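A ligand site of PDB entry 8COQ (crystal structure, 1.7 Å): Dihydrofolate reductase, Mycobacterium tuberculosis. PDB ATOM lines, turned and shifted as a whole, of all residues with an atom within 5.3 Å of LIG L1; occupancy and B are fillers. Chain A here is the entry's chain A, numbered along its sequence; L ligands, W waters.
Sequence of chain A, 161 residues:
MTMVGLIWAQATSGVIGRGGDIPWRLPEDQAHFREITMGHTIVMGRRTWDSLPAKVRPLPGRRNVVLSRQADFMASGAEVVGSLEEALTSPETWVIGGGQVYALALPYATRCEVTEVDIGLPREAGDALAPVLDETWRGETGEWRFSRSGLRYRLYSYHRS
Water W3 lies within hydrogen-bond range of N4 of LIG L1 (2.9 Å), OG1 of Thr 115 (2.9 Å), O of Glu 113 (3.0 Å) and O of Trp 8 (3.3 Å). Water W2 lies within hydrogen-bond range of the side-chain carboxylate of Asp 29, the indole nitrogen of Trp 24 and an oxygen (O1) of LIG L1.
The side-chain carboxylate of Asp 29 is in hydrogen-bond range of the side-chain hydroxyl of Thr 115 (2.7 Å). The backbone carbonyl oxygen (O) of Ile 96 lies within hydrogen-bond range of the side-chain hydroxyl (OH) of Tyr 102 (3.1 Å). O of Ile 7 sits at hydrogen-bond distance from OH of Tyr 102 (2.6 Å). The backbone carbonyl oxygen of Val 95 lies within hydrogen-bond range of the backbone NH of Ile 7. The backbone NH of Thr 115 sits at hydrogen-bond distance from the backbone carbonyl oxygen of Trp 8, at 2.9 Å. O of Glu 113 lies within hydrogen-bond range of N of Trp 8, at 3.1 Å. The backbone NH (N) of Gly 97 sits close to the side-chain hydroxyl (OH) of Tyr 102, at 3.5 Å. The backbone carbonyl oxygen of Thr 48 is in hydrogen-bond range of the side-chain hydroxyl of Ser 51 (2.6 Å).
OD1 of Asp 29 is in hydrogen-bond range of N4 of LIG L1. A nitrogen (N3) of LIG L1 lies within hydrogen-bond range of the backbone carbonyl oxygen (O) of Ile 96. N3 of LIG L1 lies within hydrogen-bond range of O of Ile 7, 3.0 Å away. N3 of LIG L1 is in hydrogen-bond range of OH of Tyr 102 (3.4 Å). An oxygen (O2) of LG2 L2 lies within hydrogen-bond range of the backbone NH (N) of Thr 48, at 3.2 Å. The side-chain hydroxyl of Thr 48 is in hydrogen-bond range of an oxygen (O2) of LG2 L2, at 2.7 Å.
Residues that only touch LIG L1: Ile 22, Trp 8, Phe 33, Gln 30, Leu 52, Thr 115, Trp 24, Ala 9 and Thr 48. Hydrophobic or aromatic side chains within 4 Å of LIG L1: Ile 7, Ala 9, Ile 22, Phe 33, Leu 52 and Ile 96. Along chain A the residues within 4 Å of LIG L1 span positions 7 to 115. The nearest printed residue that does not touch LIG L1 is Leu 59 (4.3 Å).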
ATOM      1  N   ILE A   7      -5.496  -7.242   8.969  1.00  0.00           N
ATOM      2  CA  ILE A   7      -6.210  -8.516   8.935  1.00  0.00           C
ATOM      3  C   ILE A   7      -6.887  -8.715  10.290  1.00  0.00           C
ATOM      4  O   ILE A   7      -6.264  -8.468  11.324  1.00  0.00           O
ATOM      5  CB  ILE A   7      -5.273  -9.688   8.552  1.00  0.00           C
ATOM      6  CG1 ILE A   7      -6.034 -11.026   8.509  1.00  0.00           C
ATOM      7  CG2 ILE A   7      -4.064  -9.757   9.457  1.00  0.00           C
ATOM      8  CD1 ILE A   7      -5.206 -12.157   7.866  1.00  0.00           C
ATOM      9  N   TRP A   8      -8.176  -9.080  10.268  1.00  0.00           N
ATOM     10  CA  TRP A   8      -8.914  -9.299  11.513  1.00  0.00           C
ATOM     11  C   TRP A   8     -10.087 -10.232  11.266  1.00  0.00           C
ATOM     12  O   TRP A   8     -10.544 -10.417  10.130  1.00  0.00           O
ATOM     13  CB  TRP A   8      -9.415  -7.965  12.131  1.00  0.00           C
ATOM     14  CG  TRP A   8     -10.587  -7.284  11.454  1.00  0.00           C
ATOM     15  CD1 TRP A   8     -11.905  -7.609  11.563  1.00  0.00           C
ATOM     16  CD2 TRP A   8     -10.529  -6.159  10.550  1.00  0.00           C
ATOM     17  NE1 TRP A   8     -12.677  -6.753  10.827  1.00  0.00           N
ATOM     18  CE2 TRP A   8     -11.853  -5.862  10.178  1.00  0.00           C
ATOM     19  CE3 TRP A   8      -9.488  -5.387  10.033  1.00  0.00           C
ATOM     20  CZ2 TRP A   8     -12.175  -4.812   9.320  1.00  0.00           C
ATOM     21  CZ3 TRP A   8      -9.816  -4.326   9.169  1.00  0.00           C
ATOM     22  CH2 TRP A   8     -11.144  -4.067   8.812  1.00  0.00           C
ATOM     23  N   ALA A   9     -10.592 -10.796  12.361  1.00  0.00           N
ATOM     24  CA  ALA A   9     -11.825 -11.570  12.378  1.00  0.00           C
ATOM     25  C   ALA A   9     -12.848 -10.852  13.247  1.00  0.00           C
ATOM     26  O   ALA A   9     -12.524 -10.415  14.354  1.00  0.00           O
ATOM     27  CB  ALA A   9     -11.590 -12.979  12.934  1.00  0.00           C
ATOM     28  N   ILE A  22     -10.870 -13.451  22.626  1.00  0.00           N
ATOM     29  CA  ILE A  22     -11.795 -13.554  21.470  1.00  0.00           C
ATOM     30  C   ILE A  22     -12.871 -14.583  21.792  1.00  0.00           C
ATOM     31  O   ILE A  22     -12.548 -15.630  22.224  1.00  0.00           O
ATOM     32  CB  ILE A  22     -10.992 -13.892  20.226  1.00  0.00           C
ATOM     33  CG1 ILE A  22     -10.038 -12.767  19.886  1.00  0.00           C
ATOM     34  CG2 ILE A  22     -11.912 -14.153  19.069  1.00  0.00           C
ATOM     35  CD1 ILE A  22      -8.878 -13.245  19.136  1.00  0.00           C
ATOM     36  N   TRP A  24     -14.646 -16.784  20.288  1.00  0.00           N
ATOM     37  CA  TRP A  24     -14.841 -17.854  19.310  1.00  0.00           C
ATOM     38  C   TRP A  24     -13.459 -18.391  18.970  1.00  0.00           C
ATOM     39  O   TRP A  24     -12.451 -17.811  19.350  1.00  0.00           O
ATOM     40  CB  TRP A  24     -15.557 -17.358  18.044  1.00  0.00           C
ATOM     41  CG  TRP A  24     -14.727 -16.370  17.246  1.00  0.00           C
ATOM     42  CD1 TRP A  24     -13.682 -16.639  16.421  1.00  0.00           C
ATOM     43  CD2 TRP A  24     -14.913 -14.963  17.218  1.00  0.00           C
ATOM     44  NE1 TRP A  24     -13.189 -15.468  15.877  1.00  0.00           N
ATOM     45  CE2 TRP A  24     -13.930 -14.420  16.355  1.00  0.00           C
ATOM     46  CE3 TRP A  24     -15.819 -14.089  17.832  1.00  0.00           C
ATOM     47  CZ2 TRP A  24     -13.834 -13.065  16.103  1.00  0.00           C
ATOM     48  CZ3 TRP A  24     -15.720 -12.742  17.597  1.00  0.00           C
ATOM     49  CH2 TRP A  24     -14.736 -12.244  16.730  1.00  0.00           C
ATOM     50  N   ASP A  29      -9.988 -19.910  10.202  1.00  0.00           N
ATOM     51  CA  ASP A  29      -9.498 -18.542  10.224  1.00  0.00           C
ATOM     52  C   ASP A  29      -8.046 -18.485  10.643  1.00  0.00           C
ATOM     53  O   ASP A  29      -7.270 -17.683  10.118  1.00  0.00           O
ATOM     54  CB  ASP A  29     -10.367 -17.681  11.134  1.00  0.00           C
ATOM     55  CG  ASP A  29      -9.776 -16.302  11.358  1.00  0.00           C
ATOM     56  OD1 ASP A  29      -9.701 -15.531  10.370  1.00  0.00           O
ATOM     57  OD2 ASP A  29      -9.374 -15.998  12.486  1.00  0.00           O
ATOM     58  N   GLN A  30      -7.643 -19.323  11.604  1.00  0.00           N
ATOM     59  CA  GLN A  30      -6.228 -19.340  11.986  1.00  0.00           C
ATOM     60  C   GLN A  30      -5.341 -19.724  10.807  1.00  0.00           C
ATOM     61  O   GLN A  30      -4.260 -19.155  10.620  1.00  0.00           O
ATOM     62  CB  GLN A  30      -6.004 -20.275  13.171  1.00  0.00           C
ATOM     63  CG  GLN A  30      -6.548 -19.706  14.471  1.00  0.00           C
ATOM     64  CD  GLN A  30      -6.254 -20.606  15.673  1.00  0.00           C
ATOM     65  OE1 GLN A  30      -7.160 -20.939  16.449  1.00  0.00           O
ATOM     66  NE2 GLN A  30      -5.000 -21.060  15.776  1.00  0.00           N
ATOM     67  N   HIS A  32      -6.037 -19.220   7.589  1.00  0.00           N
ATOM     68  CA  HIS A  32      -6.025 -18.096   6.660  1.00  0.00           C
ATOM     69  C   HIS A  32      -5.088 -16.993   7.174  1.00  0.00           C
ATOM     70  O   HIS A  32      -4.268 -16.457   6.413  1.00  0.00           O
ATOM     71  CB  HIS A  32      -7.457 -17.591   6.508  1.00  0.00           C
ATOM     72  CG  HIS A  32      -7.594 -16.313   5.753  1.00  0.00           C
ATOM     73  ND1 HIS A  32      -7.381 -16.240   4.398  1.00  0.00           N
ATOM     74  CD2 HIS A  32      -7.953 -15.068   6.146  1.00  0.00           C
ATOM     75  CE1 HIS A  32      -7.575 -15.002   3.991  1.00  0.00           C
ATOM     76  NE2 HIS A  32      -7.932 -14.271   5.031  1.00  0.00           N
ATOM     77  N   PHE A  33      -5.160 -16.709   8.489  1.00  0.00           N
ATOM     78  CA  PHE A  33      -4.257 -15.736   9.114  1.00  0.00           C
ATOM     79  C   PHE A  33      -2.804 -16.122   8.921  1.00  0.00           C
ATOM     80  O   PHE A  33      -1.965 -15.277   8.575  1.00  0.00           O
ATOM     81  CB  PHE A  33      -4.580 -15.618  10.595  1.00  0.00           C
ATOM     82  CG  PHE A  33      -3.589 -14.812  11.368  1.00  0.00           C
ATOM     83  CD1 PHE A  33      -3.699 -13.422  11.414  1.00  0.00           C
ATOM     84  CD2 PHE A  33      -2.550 -15.423  12.035  1.00  0.00           C
ATOM     85  CE1 PHE A  33      -2.783 -12.664  12.119  1.00  0.00           C
ATOM     86  CE2 PHE A  33      -1.628 -14.676  12.746  1.00  0.00           C
ATOM     87  CZ  PHE A  33      -1.756 -13.282  12.785  1.00  0.00           C
ATOM     88  N   THR A  48      -2.532  -6.862  22.663  1.00  0.00           N
ATOM     89  CA  THR A  48      -2.639  -8.092  21.887  1.00  0.00           C
ATOM     90  C   THR A  48      -1.444  -9.019  22.113  1.00  0.00           C
ATOM     91  O   THR A  48      -1.608 -10.242  22.202  1.00  0.00           O
ATOM     92  CB  THR A  48      -2.842  -7.765  20.411  1.00  0.00           C
ATOM     93  OG1 THR A  48      -4.142  -7.163  20.267  1.00  0.00           O
ATOM     94  CG2 THR A  48      -2.741  -9.038  19.499  1.00  0.00           C
ATOM     95  N   SER A  51      -1.964 -10.906  25.123  1.00  0.00           N
ATOM     96  CA  SER A  51      -2.984 -11.942  24.983  1.00  0.00           C
ATOM     97  C   SER A  51      -2.399 -13.254  24.503  1.00  0.00           C
ATOM     98  O   SER A  51      -3.027 -14.311  24.705  1.00  0.00           O
ATOM     99  CB  SER A  51      -4.097 -11.462  24.048  1.00  0.00           C
ATOM    100  OG  SER A  51      -3.749 -11.641  22.689  1.00  0.00           O
ATOM    101  N   LEU A  52      -1.216 -13.220  23.894  1.00  0.00           N
ATOM    102  CA  LEU A  52      -0.509 -14.416  23.434  1.00  0.00           C
ATOM    103  C   LEU A  52       0.181 -15.109  24.606  1.00  0.00           C
ATOM    104  O   LEU A  52       0.961 -14.473  25.324  1.00  0.00           O
ATOM    105  CB  LEU A  52       0.516 -14.048  22.376  1.00  0.00           C
ATOM    106  CG  LEU A  52      -0.013 -13.378  21.113  1.00  0.00           C
ATOM    107  CD1 LEU A  52       1.113 -13.060  20.160  1.00  0.00           C
ATOM    108  CD2 LEU A  52      -0.943 -14.389  20.474  1.00  0.00           C
ATOM    109  N   LEU A  59       5.336 -15.145  16.953  1.00  0.00           N
ATOM    110  CA  LEU A  59       4.808 -15.985  15.877  1.00  0.00           C
ATOM    111  C   LEU A  59       5.956 -16.329  14.933  1.00  0.00           C
ATOM    112  O   LEU A  59       6.568 -15.463  14.448  1.00  0.00           O
ATOM    113  CB  LEU A  59       3.727 -15.173  15.194  1.00  0.00           C
ATOM    114  CG  LEU A  59       2.358 -15.315  15.840  1.00  0.00           C
ATOM    115  CD1 LEU A  59       2.432 -15.114  17.320  1.00  0.00           C
ATOM    116  CD2 LEU A  59       1.331 -14.402  15.231  1.00  0.00           C
ATOM    117  N   VAL A  95      -0.897  -5.487   9.921  1.00  0.00           N
ATOM    118  CA  VAL A  95      -1.355  -5.080  11.233  1.00  0.00           C
ATOM    119  C   VAL A  95      -2.355  -6.119  11.692  1.00  0.00           C
ATOM    120  O   VAL A  95      -3.362  -6.334  11.017  1.00  0.00           O
ATOM    121  CB  VAL A  95      -2.007  -3.703  11.187  1.00  0.00           C
ATOM    122  CG1 VAL A  95      -2.502  -3.312  12.585  1.00  0.00           C
ATOM    123  CG2 VAL A  95      -1.013  -2.661  10.658  1.00  0.00           C
ATOM    124  N   ILE A  96      -2.065  -6.762  12.820  1.00  0.00           N
ATOM    125  CA  ILE A  96      -2.836  -7.926  13.261  1.00  0.00           C
ATOM    126  C   ILE A  96      -3.648  -7.648  14.516  1.00  0.00           C
ATOM    127  O   ILE A  96      -4.199  -8.580  15.114  1.00  0.00           O
ATOM    128  CB  ILE A  96      -1.948  -9.164  13.473  1.00  0.00           C
ATOM    129  CG1 ILE A  96      -1.017  -8.972  14.672  1.00  0.00           C
ATOM    130  CG2 ILE A  96      -1.139  -9.410  12.248  1.00  0.00           C
ATOM    131  CD1 ILE A  96      -0.194 -10.252  14.994  1.00  0.00           C
ATOM    132  N   GLY A  97      -3.758  -6.391  14.929  1.00  0.00           N
ATOM    133  CA  GLY A  97      -4.655  -6.009  16.017  1.00  0.00           C
ATOM    134  C   GLY A  97      -3.904  -5.432  17.197  1.00  0.00           C
ATOM    135  O   GLY A  97      -2.678  -5.417  17.234  1.00  0.00           O
ATOM    136  N   TYR A 102      -5.670  -1.115  14.880  1.00  0.00           N
ATOM    137  CA  TYR A 102      -6.415  -1.062  13.621  1.00  0.00           C
ATOM    138  C   TYR A 102      -6.783   0.375  13.284  1.00  0.00           C
ATOM    139  O   TYR A 102      -6.525   0.848  12.167  1.00  0.00           O
ATOM    140  CB  TYR A 102      -7.674  -1.916  13.707  1.00  0.00           C
ATOM    141  CG  TYR A 102      -7.411  -3.400  13.688  1.00  0.00           C
ATOM    142  CD1 TYR A 102      -8.147  -4.252  14.502  1.00  0.00           C
ATOM    143  CD2 TYR A 102      -6.449  -3.964  12.850  1.00  0.00           C
ATOM    144  CE1 TYR A 102      -7.928  -5.611  14.508  1.00  0.00           C
ATOM    145  CE2 TYR A 102      -6.219  -5.342  12.844  1.00  0.00           C
ATOM    146  CZ  TYR A 102      -6.985  -6.154  13.678  1.00  0.00           C
ATOM    147  OH  TYR A 102      -6.795  -7.510  13.731  1.00  0.00           O
ATOM    148  N   GLU A 113      -8.028  -7.697   5.037  1.00  0.00           N
ATOM    149  CA  GLU A 113      -8.474  -9.072   4.896  1.00  0.00           C
ATOM    150  C   GLU A 113      -9.355  -9.395   6.099  1.00  0.00           C
ATOM    151  O   GLU A 113      -8.855  -9.484   7.226  1.00  0.00           O
ATOM    152  CB  GLU A 113      -7.276 -10.029   4.811  1.00  0.00           C
ATOM    153  CG  GLU A 113      -6.459  -9.848   3.536  1.00  0.00           C
ATOM    154  CD  GLU A 113      -7.206 -10.320   2.302  1.00  0.00           C
ATOM    155  OE1 GLU A 113      -8.033 -11.250   2.419  1.00  0.00           O
ATOM    156  OE2 GLU A 113      -6.959  -9.770   1.207  1.00  0.00           O
ATOM    157  N   THR A 115     -12.270 -11.656   8.120  1.00  0.00           N
ATOM    158  CA  THR A 115     -13.106 -12.825   8.355  1.00  0.00           C
ATOM    159  C   THR A 115     -14.344 -12.400   9.128  1.00  0.00           C
ATOM    160  O   THR A 115     -14.238 -11.869  10.235  1.00  0.00           O
ATOM    161  CB  THR A 115     -12.341 -13.899   9.135  1.00  0.00           C
ATOM    162  OG1 THR A 115     -11.151 -14.259   8.445  1.00  0.00           O
ATOM    163  CG2 THR A 115     -13.230 -15.146   9.342  1.00  0.00           C
HETATM  164  C1  LIG L   1      -7.450 -16.218  16.626  1.00  0.00           C
HETATM  165  C2  LIG L   1      -5.275 -15.864  14.869  1.00  0.00           C
HETATM  166  C3  LIG L   1      -3.254 -12.901  18.408  1.00  0.00           C
HETATM  167  C4  LIG L   1      -7.555 -13.007  11.790  1.00  0.00           C
HETATM  168  C5  LIG L   1      -6.569 -13.901  13.798  1.00  0.00           C
HETATM  169  C6  LIG L   1      -5.899 -12.730  14.019  1.00  0.00           C
HETATM  170  C7  LIG L   1      -6.120 -11.765  13.045  1.00  0.00           C
HETATM  171  C8  LIG L   1      -4.961 -12.458  15.198  1.00  0.00           C
HETATM  172  C9  LIG L   1      -4.223 -12.230  16.094  1.00  0.00           C
HETATM  173  C10 LIG L   1      -3.283 -11.898  17.250  1.00  0.00           C
HETATM  174  C11 LIG L   1      -6.404 -15.048  14.796  1.00  0.00           C
HETATM  175  C12 LIG L   1      -7.476 -15.214  15.658  1.00  0.00           C
HETATM  176  C13 LIG L   1      -6.330 -17.031  16.694  1.00  0.00           C
HETATM  177  C14 LIG L   1      -5.249 -16.868  15.836  1.00  0.00           C
HETATM  178  C15 LIG L   1      -9.700 -14.469  16.257  1.00  0.00           C
HETATM  179  C16 LIG L   1      -2.101 -12.865  17.366  1.00  0.00           C
HETATM  180  N1  LIG L   1      -6.894 -11.876  11.979  1.00  0.00           N
HETATM  181  N2  LIG L   1      -7.351 -13.951  12.738  1.00  0.00           N
HETATM  182  N3  LIG L   1      -5.398 -10.526  13.264  1.00  0.00           N
HETATM  183  N4  LIG L   1      -8.453 -13.238  10.649  1.00  0.00           N
HETATM  184  O1  LIG L   1      -8.538 -14.297  15.452  1.00  0.00           O
HETATM  185  P1  LG2 L   2      -4.420  -3.228  21.341  1.00  0.00           P
HETATM  186  O1  LG2 L   2      -4.811  -2.397  20.230  1.00  0.00           O
HETATM  187  O2  LG2 L   2      -4.055  -4.584  21.029  1.00  0.00           O
HETATM  188  O3  LG2 L   2      -3.282  -2.571  22.173  1.00  0.00           O
HETATM  189  C1  LG2 L   2      -3.421  -1.236  22.657  1.00  0.00           C
HETATM  190  C2  LG2 L   2      -2.099  -0.788  23.247  1.00  0.00           C
HETATM  191  O4  LG2 L   2      -1.177  -0.528  22.181  1.00  0.00           O
HETATM  192  C3  LG2 L   2      -2.061   0.487  24.085  1.00  0.00           C
HETATM  193  O5  LG2 L   2      -2.333   0.119  25.422  1.00  0.00           O
HETATM  194  C4  LG2 L   2      -0.598   0.873  23.957  1.00  0.00           C
HETATM  195  O6  LG2 L   2       0.223   0.031  24.691  1.00  0.00           O
HETATM  196  C5  LG2 L   2      -0.354   0.556  22.491  1.00  0.00           C
HETATM  197  N1  LG2 L   2      -0.652   1.681  21.621  1.00  0.00           N
HETATM  198  C6  LG2 L   2      -1.855   2.078  21.175  1.00  0.00           C
HETATM  199  N2  LG2 L   2      -1.818   3.149  20.432  1.00  0.00           N
HETATM  200  C7  LG2 L   2      -0.489   3.501  20.427  1.00  0.00           C
HETATM  201  C8  LG2 L   2       0.207   4.554  19.820  1.00  0.00           C
HETATM  202  N3  LG2 L   2      -0.363   5.509  19.111  1.00  0.00           N
HETATM  203  N4  LG2 L   2       1.534   4.615  20.023  1.00  0.00           N
HETATM  204  C9  LG2 L   2       2.117   3.667  20.734  1.00  0.00           C
HETATM  205  N5  LG2 L   2       1.560   2.625  21.330  1.00  0.00           N
HETATM  206  C10 LG2 L   2       0.244   2.600  21.149  1.00  0.00           C
HETATM  207  O7  LG2 L   2      -5.600  -3.244  22.379  1.00  0.00           O
HETATM  208  P2  LG2 L   2      -7.152  -3.399  22.207  1.00  0.00           P
HETATM  209  O8  LG2 L   2      -7.694  -2.402  21.343  1.00  0.00           O
HETATM  210  O9  LG2 L   2      -7.747  -3.473  23.523  1.00  0.00           O
HETATM  211  O10 LG2 L   2      -7.333  -4.782  21.496  1.00  0.00           O
HETATM  212  C11 LG2 L   2      -7.114  -5.969  22.213  1.00  0.00           C
HETATM  213  C12 LG2 L   2      -8.243  -6.922  21.953  1.00  0.00           C
HETATM  214  O11 LG2 L   2      -8.382  -7.220  20.550  1.00  0.00           O
HETATM  215  C13 LG2 L   2      -8.163  -8.283  22.658  1.00  0.00           C
HETATM  216  O12 LG2 L   2      -9.475  -8.731  22.954  1.00  0.00           O
HETATM  217  C14 LG2 L   2      -7.667  -9.156  21.537  1.00  0.00           C
HETATM  218  O13 LG2 L   2      -7.910 -10.507  21.801  1.00  0.00           O
HETATM  219  C15 LG2 L   2      -8.506  -8.610  20.395  1.00  0.00           C
HETATM  220  N6  LG2 L   2      -7.987  -9.026  19.092  1.00  0.00           N
HETATM  221  C16 LG2 L   2      -8.799  -9.527  18.120  1.00  0.00           C
HETATM  222  C17 LG2 L   2      -8.334  -9.883  16.911  1.00  0.00           C
HETATM  223  C18 LG2 L   2      -9.258 -10.394  15.878  1.00  0.00           C
HETATM  224  O14 LG2 L   2     -10.395 -10.719  16.173  1.00  0.00           O
HETATM  225  N7  LG2 L   2      -8.811 -10.503  14.652  1.00  0.00           N
HETATM  226  C19 LG2 L   2      -6.914  -9.779  16.675  1.00  0.00           C
HETATM  227  C20 LG2 L   2      -6.139  -9.173  17.728  1.00  0.00           C
HETATM  228  C21 LG2 L   2      -6.676  -8.869  18.860  1.00  0.00           C
HETATM  229  P3  LG2 L   2       0.806   0.479  26.078  1.00  0.00           P
HETATM  230  O15 LG2 L   2       1.793  -0.493  26.410  1.00  0.00           O
HETATM  231  O16 LG2 L   2       1.318   1.775  25.823  1.00  0.00           O
HETATM  232  O17 LG2 L   2      -0.305   0.468  27.000  1.00  0.00           O
HETATM  233  O   HOH W   1      -9.980 -18.505  15.872  1.00  0.00           O
HETATM  234  O   HOH W   2     -10.900 -16.630  14.574  1.00  0.00           O
HETATM  235  O   HOH W   3      -9.000 -12.383   7.965  1.00  0.00           O
